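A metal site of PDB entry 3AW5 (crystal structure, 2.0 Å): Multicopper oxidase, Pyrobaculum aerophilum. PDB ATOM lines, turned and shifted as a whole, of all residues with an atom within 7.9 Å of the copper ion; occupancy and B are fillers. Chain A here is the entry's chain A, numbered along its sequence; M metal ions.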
ATOM      1  N   ILE A 164      -3.524  16.098 -25.823  1.00  0.00           N
ATOM      2  CA  ILE A 164      -2.481  15.402 -25.085  1.00  0.00           C
ATOM      3  C   ILE A 164      -2.698  13.889 -25.126  1.00  0.00           C
ATOM      4  O   ILE A 164      -1.753  13.118 -25.342  1.00  0.00           O
ATOM      5  CB  ILE A 164      -2.450  15.814 -23.604  1.00  0.00           C
ATOM      6  CG1 ILE A 164      -2.068  17.293 -23.472  1.00  0.00           C
ATOM      7  CG2 ILE A 164      -1.502  14.914 -22.820  1.00  0.00           C
ATOM      8  CD1 ILE A 164      -0.726  17.624 -24.049  1.00  0.00           C
ATOM      9  N   ALA A 165      -3.938  13.462 -24.931  1.00  0.00           N
ATOM     10  CA  ALA A 165      -4.222  12.018 -24.885  1.00  0.00           C
ATOM     11  C   ALA A 165      -4.591  11.350 -26.212  1.00  0.00           C
ATOM     12  O   ALA A 165      -4.407  10.143 -26.369  1.00  0.00           O
ATOM     13  CB  ALA A 165      -5.329  11.769 -23.867  1.00  0.00           C
ATOM     14  N   LEU A 319      10.784   8.919 -25.261  1.00  0.00           N
ATOM     15  CA  LEU A 319       9.476   9.488 -25.557  1.00  0.00           C
ATOM     16  C   LEU A 319       8.942  10.006 -24.227  1.00  0.00           C
ATOM     17  O   LEU A 319       8.729   9.219 -23.303  1.00  0.00           O
ATOM     18  CB  LEU A 319       8.544   8.408 -26.128  1.00  0.00           C
ATOM     19  CG  LEU A 319       9.123   7.611 -27.299  1.00  0.00           C
ATOM     20  CD1 LEU A 319       8.041   6.633 -27.835  1.00  0.00           C
ATOM     21  CD2 LEU A 319       9.575   8.583 -28.401  1.00  0.00           C
ATOM     22  N   TRP A 326       4.541  16.893 -26.176  1.00  0.00           N
ATOM     23  CA  TRP A 326       5.121  15.555 -26.347  1.00  0.00           C
ATOM     24  C   TRP A 326       6.461  15.748 -27.058  1.00  0.00           C
ATOM     25  O   TRP A 326       6.566  16.540 -27.984  1.00  0.00           O
ATOM     26  CB  TRP A 326       4.214  14.649 -27.186  1.00  0.00           C
ATOM     27  CG  TRP A 326       3.079  14.064 -26.430  1.00  0.00           C
ATOM     28  CD1 TRP A 326       1.764  14.380 -26.555  1.00  0.00           C
ATOM     29  CD2 TRP A 326       3.145  13.016 -25.449  1.00  0.00           C
ATOM     30  NE1 TRP A 326       1.004  13.602 -25.708  1.00  0.00           N
ATOM     31  CE2 TRP A 326       1.831  12.760 -25.026  1.00  0.00           C
ATOM     32  CE3 TRP A 326       4.201  12.270 -24.888  1.00  0.00           C
ATOM     33  CZ2 TRP A 326       1.523  11.783 -24.064  1.00  0.00           C
ATOM     34  CZ3 TRP A 326       3.903  11.306 -23.929  1.00  0.00           C
ATOM     35  CH2 TRP A 326       2.574  11.063 -23.530  1.00  0.00           C
ATOM     36  N   ASN A 355       9.901   4.365 -24.030  1.00  0.00           N
ATOM     37  CA  ASN A 355       8.732   5.164 -23.672  1.00  0.00           C
ATOM     38  C   ASN A 355       8.717   5.331 -22.141  1.00  0.00           C
ATOM     39  O   ASN A 355       8.866   4.349 -21.397  1.00  0.00           O
ATOM     40  CB  ASN A 355       7.451   4.490 -24.180  1.00  0.00           C
ATOM     41  CG  ASN A 355       6.224   5.399 -24.128  1.00  0.00           C
ATOM     42  OD1 ASN A 355       6.326   6.572 -23.750  1.00  0.00           O
ATOM     43  ND2 ASN A 355       5.065   4.862 -24.505  1.00  0.00           N
ATOM     44  N   SER A 359       3.561   7.883 -19.281  1.00  0.00           N
ATOM     45  CA  SER A 359       3.282   8.215 -20.677  1.00  0.00           C
ATOM     46  C   SER A 359       2.145   7.298 -21.124  1.00  0.00           C
ATOM     47  O   SER A 359       1.487   6.688 -20.299  1.00  0.00           O
ATOM     48  CB  SER A 359       4.552   7.962 -21.500  1.00  0.00           C
ATOM     49  OG  SER A 359       4.404   8.298 -22.871  1.00  0.00           O
ATOM     50  N   MET A 360       1.901   7.247 -22.431  1.00  0.00           N
ATOM     51  CA  MET A 360       0.867   6.387 -22.968  1.00  0.00           C
ATOM     52  C   MET A 360       1.480   5.646 -24.164  1.00  0.00           C
ATOM     53  O   MET A 360       2.555   5.988 -24.621  1.00  0.00           O
ATOM     54  CB  MET A 360      -0.352   7.209 -23.395  1.00  0.00           C
ATOM     55  CG  MET A 360      -0.067   8.296 -24.396  1.00  0.00           C
ATOM     56  SD  MET A 360      -1.584   9.104 -24.943  1.00  0.00           S
ATOM     57  CE  MET A 360      -2.154   7.880 -26.231  1.00  0.00           C
ATOM     58  N   PRO A 361       0.805   4.601 -24.657  1.00  0.00           N
ATOM     59  CA  PRO A 361       1.384   3.882 -25.803  1.00  0.00           C
ATOM     60  C   PRO A 361       1.517   4.813 -27.019  1.00  0.00           C
ATOM     61  O   PRO A 361       0.602   5.589 -27.288  1.00  0.00           O
ATOM     62  CB  PRO A 361       0.388   2.755 -26.058  1.00  0.00           C
ATOM     63  CG  PRO A 361      -0.320   2.586 -24.733  1.00  0.00           C
ATOM     64  CD  PRO A 361      -0.476   3.995 -24.236  1.00  0.00           C
ATOM     65  N   HIS A 362       2.646   4.739 -27.722  1.00  0.00           N
ATOM     66  CA  HIS A 362       2.867   5.578 -28.903  1.00  0.00           C
ATOM     67  C   HIS A 362       3.225   4.739 -30.131  1.00  0.00           C
ATOM     68  O   HIS A 362       4.200   3.981 -30.101  1.00  0.00           O
ATOM     69  CB  HIS A 362       4.039   6.551 -28.703  1.00  0.00           C
ATOM     70  CG  HIS A 362       3.862   7.520 -27.569  1.00  0.00           C
ATOM     71  ND1 HIS A 362       2.982   8.572 -27.627  1.00  0.00           N
ATOM     72  CD2 HIS A 362       4.479   7.615 -26.372  1.00  0.00           C
ATOM     73  CE1 HIS A 362       3.074   9.288 -26.524  1.00  0.00           C
ATOM     74  NE2 HIS A 362       3.978   8.726 -25.737  1.00  0.00           N
ATOM     75  N   PRO A 363       2.444   4.853 -31.219  1.00  0.00           N
ATOM     76  CA  PRO A 363       2.782   4.065 -32.416  1.00  0.00           C
ATOM     77  C   PRO A 363       3.769   4.929 -33.211  1.00  0.00           C
ATOM     78  O   PRO A 363       3.363   5.865 -33.894  1.00  0.00           O
ATOM     79  CB  PRO A 363       1.431   3.892 -33.108  1.00  0.00           C
ATOM     80  CG  PRO A 363       0.709   5.206 -32.762  1.00  0.00           C
ATOM     81  CD  PRO A 363       1.087   5.425 -31.310  1.00  0.00           C
ATOM     82  N   MET A 364       5.061   4.629 -33.089  1.00  0.00           N
ATOM     83  CA  MET A 364       6.078   5.420 -33.765  1.00  0.00           C
ATOM     84  C   MET A 364       6.276   4.961 -35.204  1.00  0.00           C
ATOM     85  O   MET A 364       6.415   3.769 -35.471  1.00  0.00           O
ATOM     86  CB  MET A 364       7.399   5.378 -32.997  1.00  0.00           C
ATOM     87  CG  MET A 364       7.314   5.985 -31.571  1.00  0.00           C
ATOM     88  SD  MET A 364       6.680   7.696 -31.520  1.00  0.00           S
ATOM     89  CE  MET A 364       8.008   8.591 -32.308  1.00  0.00           C
ATOM     90  N   LEU A 405       4.292   0.006 -32.117  1.00  0.00           N
ATOM     91  CA  LEU A 405       3.743   0.480 -30.840  1.00  0.00           C
ATOM     92  C   LEU A 405       4.682   0.248 -29.668  1.00  0.00           C
ATOM     93  O   LEU A 405       5.191  -0.853 -29.479  1.00  0.00           O
ATOM     94  CB  LEU A 405       2.426  -0.248 -30.526  1.00  0.00           C
ATOM     95  CG  LEU A 405       1.654   0.291 -29.316  1.00  0.00           C
ATOM     96  CD1 LEU A 405       1.314   1.779 -29.533  1.00  0.00           C
ATOM     97  CD2 LEU A 405       0.366  -0.516 -29.128  1.00  0.00           C
ATOM     98  N   ILE A 406       4.919   1.299 -28.895  1.00  0.00           N
ATOM     99  CA  ILE A 406       5.780   1.205 -27.718  1.00  0.00           C
ATOM    100  C   ILE A 406       4.942   1.625 -26.515  1.00  0.00           C
ATOM    101  O   ILE A 406       4.410   2.748 -26.462  1.00  0.00           O
ATOM    102  CB  ILE A 406       7.041   2.102 -27.821  1.00  0.00           C
ATOM    103  CG1 ILE A 406       7.873   1.731 -29.055  1.00  0.00           C
ATOM    104  CG2 ILE A 406       7.924   1.875 -26.590  1.00  0.00           C
ATOM    105  CD1 ILE A 406       7.816   2.741 -30.178  1.00  0.00           C
ATOM    106  N   HIS A 430       7.855  10.205 -36.348  1.00  0.00           N
ATOM    107  CA  HIS A 430       6.840  10.760 -35.461  1.00  0.00           C
ATOM    108  C   HIS A 430       5.860   9.737 -34.925  1.00  0.00           C
ATOM    109  O   HIS A 430       5.851   8.566 -35.348  1.00  0.00           O
ATOM    110  CB  HIS A 430       6.045  11.821 -36.228  1.00  0.00           C
ATOM    111  CG  HIS A 430       5.233  11.259 -37.355  1.00  0.00           C
ATOM    112  ND1 HIS A 430       3.941  10.827 -37.192  1.00  0.00           N
ATOM    113  CD2 HIS A 430       5.556  11.019 -38.647  1.00  0.00           C
ATOM    114  CE1 HIS A 430       3.493  10.351 -38.341  1.00  0.00           C
ATOM    115  NE2 HIS A 430       4.454  10.450 -39.236  1.00  0.00           N
ATOM    116  N   CYS A 431       5.046  10.181 -33.982  1.00  0.00           N
ATOM    117  CA  CYS A 431       4.038   9.305 -33.430  1.00  0.00           C
ATOM    118  C   CYS A 431       2.875   9.390 -34.395  1.00  0.00           C
ATOM    119  O   CYS A 431       2.598  10.461 -34.934  1.00  0.00           O
ATOM    120  CB  CYS A 431       3.586   9.777 -32.042  1.00  0.00           C
ATOM    121  SG  CYS A 431       2.263   8.757 -31.436  1.00  0.00           S
ATOM    122  N   HIS A 432       2.200   8.270 -34.613  1.00  0.00           N
ATOM    123  CA  HIS A 432       1.081   8.273 -35.544  1.00  0.00           C
ATOM    124  C   HIS A 432      -0.269   8.516 -34.897  1.00  0.00           C
ATOM    125  O   HIS A 432      -1.316   8.353 -35.535  1.00  0.00           O
ATOM    126  CB  HIS A 432       1.046   6.991 -36.376  1.00  0.00           C
ATOM    127  CG  HIS A 432       0.537   7.231 -37.760  1.00  0.00           C
ATOM    128  ND1 HIS A 432      -0.794   7.499 -38.017  1.00  0.00           N
ATOM    129  CD2 HIS A 432       1.178   7.329 -38.944  1.00  0.00           C
ATOM    130  CE1 HIS A 432      -0.938   7.756 -39.312  1.00  0.00           C
ATOM    131  NE2 HIS A 432       0.242   7.667 -39.892  1.00  0.00           N
ATOM    132  N   ASN A 433      -0.249   8.876 -33.613  1.00  0.00           N
ATOM    133  CA  ASN A 433      -1.464   9.274 -32.901  1.00  0.00           C
ATOM    134  C   ASN A 433      -1.544  10.677 -33.520  1.00  0.00           C
ATOM    135  O   ASN A 433      -0.674  11.511 -33.270  1.00  0.00           O
ATOM    136  CB  ASN A 433      -1.184   9.338 -31.389  1.00  0.00           C
ATOM    137  CG  ASN A 433      -2.281  10.045 -30.605  1.00  0.00           C
ATOM    138  OD1 ASN A 433      -2.729  11.123 -30.991  1.00  0.00           O
ATOM    139  ND2 ASN A 433      -2.712   9.449 -29.508  1.00  0.00           N
ATOM    140  N   LEU A 434      -2.553  10.946 -34.339  1.00  0.00           N
ATOM    141  CA  LEU A 434      -2.612  12.232 -35.020  1.00  0.00           C
ATOM    142  C   LEU A 434      -2.699  13.484 -34.141  1.00  0.00           C
ATOM    143  O   LEU A 434      -2.254  14.546 -34.552  1.00  0.00           O
ATOM    144  CB  LEU A 434      -3.730  12.218 -36.056  1.00  0.00           C
ATOM    145  CG  LEU A 434      -3.559  11.062 -37.075  1.00  0.00           C
ATOM    146  CD1 LEU A 434      -4.629  11.185 -38.150  1.00  0.00           C
ATOM    147  CD2 LEU A 434      -2.173  11.110 -37.705  1.00  0.00           C
ATOM    148  N   GLU A 435      -3.257  13.359 -32.937  1.00  0.00           N
ATOM    149  CA  GLU A 435      -3.312  14.523 -32.052  1.00  0.00           C
ATOM    150  C   GLU A 435      -1.883  14.795 -31.566  1.00  0.00           C
ATOM    151  O   GLU A 435      -1.455  15.948 -31.479  1.00  0.00           O
ATOM    152  CB  GLU A 435      -4.257  14.263 -30.860  1.00  0.00           C
ATOM    153  CG  GLU A 435      -5.754  14.415 -31.200  1.00  0.00           C
ATOM    154  CD  GLU A 435      -6.249  13.376 -32.204  1.00  0.00           C
ATOM    155  OE1 GLU A 435      -6.158  12.166 -31.907  1.00  0.00           O
ATOM    156  OE2 GLU A 435      -6.733  13.753 -33.292  1.00  0.00           O
ATOM    157  N   HIS A 436      -1.127  13.732 -31.278  1.00  0.00           N
ATOM    158  CA  HIS A 436       0.261  13.900 -30.840  1.00  0.00           C
ATOM    159  C   HIS A 436       1.075  14.489 -31.994  1.00  0.00           C
ATOM    160  O   HIS A 436       1.892  15.397 -31.805  1.00  0.00           O
ATOM    161  CB  HIS A 436       0.872  12.556 -30.405  1.00  0.00           C
ATOM    162  CG  HIS A 436       0.254  11.993 -29.152  1.00  0.00           C
ATOM    163  ND1 HIS A 436       0.669  10.812 -28.589  1.00  0.00           N
ATOM    164  CD2 HIS A 436      -0.760  12.444 -28.365  1.00  0.00           C
ATOM    165  CE1 HIS A 436      -0.051  10.542 -27.522  1.00  0.00           C
ATOM    166  NE2 HIS A 436      -0.931  11.522 -27.359  1.00  0.00           N
ATOM    167  N   GLU A 437       0.842  13.974 -33.203  1.00  0.00           N
ATOM    168  CA  GLU A 437       1.543  14.456 -34.386  1.00  0.00           C
ATOM    169  C   GLU A 437       1.279  15.941 -34.600  1.00  0.00           C
ATOM    170  O   GLU A 437       2.212  16.734 -34.740  1.00  0.00           O
ATOM    171  CB  GLU A 437       1.113  13.666 -35.619  1.00  0.00           C
ATOM    172  CG  GLU A 437       1.944  13.992 -36.851  1.00  0.00           C
ATOM    173  CD  GLU A 437       1.435  13.275 -38.077  1.00  0.00           C
ATOM    174  OE1 GLU A 437       1.113  12.073 -37.977  1.00  0.00           O
ATOM    175  OE2 GLU A 437       1.361  13.909 -39.150  1.00  0.00           O
ATOM    176  N   MET A 441       4.765  16.097 -31.974  1.00  0.00           N
ATOM    177  CA  MET A 441       5.593  14.924 -31.685  1.00  0.00           C
ATOM    178  C   MET A 441       6.072  14.364 -33.025  1.00  0.00           C
ATOM    179  O   MET A 441       5.658  13.283 -33.449  1.00  0.00           O
ATOM    180  CB  MET A 441       4.795  13.868 -30.907  1.00  0.00           C
ATOM    181  CG  MET A 441       5.661  12.843 -30.171  1.00  0.00           C
ATOM    182  SD  MET A 441       4.682  11.685 -29.146  1.00  0.00           S
ATOM    183  CE  MET A 441       5.982  10.645 -28.428  1.00  0.00           C
HETATM  184 CU    CU M   1       2.066   9.384 -29.357  1.00  0.00          CU
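The copper ion is bound by a ring nitrogen (ND1) of His 362, a ring nitrogen (ND1) of His 436 and the side-chain sulfur (SG) of Cys 431.
Asn 433 touches the copper ion (CB to CU, 3.8 Å).
Met 441 touches the copper ion (SD to CU, 3.5 Å).
The nearest printed residue that does not touch the copper ion is Pro 363 (4.5 Å).
NE2 of His 362 is in hydrogen-bond range of OG of Ser 359 (2.9 Å).
The backbone carbonyl oxygen of Ile 406 is in hydrogen-bond range of the backbone NH of His 362, at 2.9 Å.
The backbone carbonyl oxygen (O) of His 436 sits at hydrogen-bond distance from the backbone NH (N) of Met 441 (3.0 Å).
The backbone NH (N) of His 436 sits at hydrogen-bond distance from the side-chain amide oxygen (OD1) of Asn 433.
A ring nitrogen (NE2) of His 436 lies close to the side-chain sulfur of Met 360 (3.5 Å).
NE2 of His 436 lies within hydrogen-bond range of O of Ile 164, 2.7 Å away.
SG of Cys 431 lies close to N of Asn 433 (3.3 Å).
The backbone NH (N) of Glu 435 is in hydrogen-bond range of the side-chain amide oxygen (OD1) of Asn 433, at 3.0 Å.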
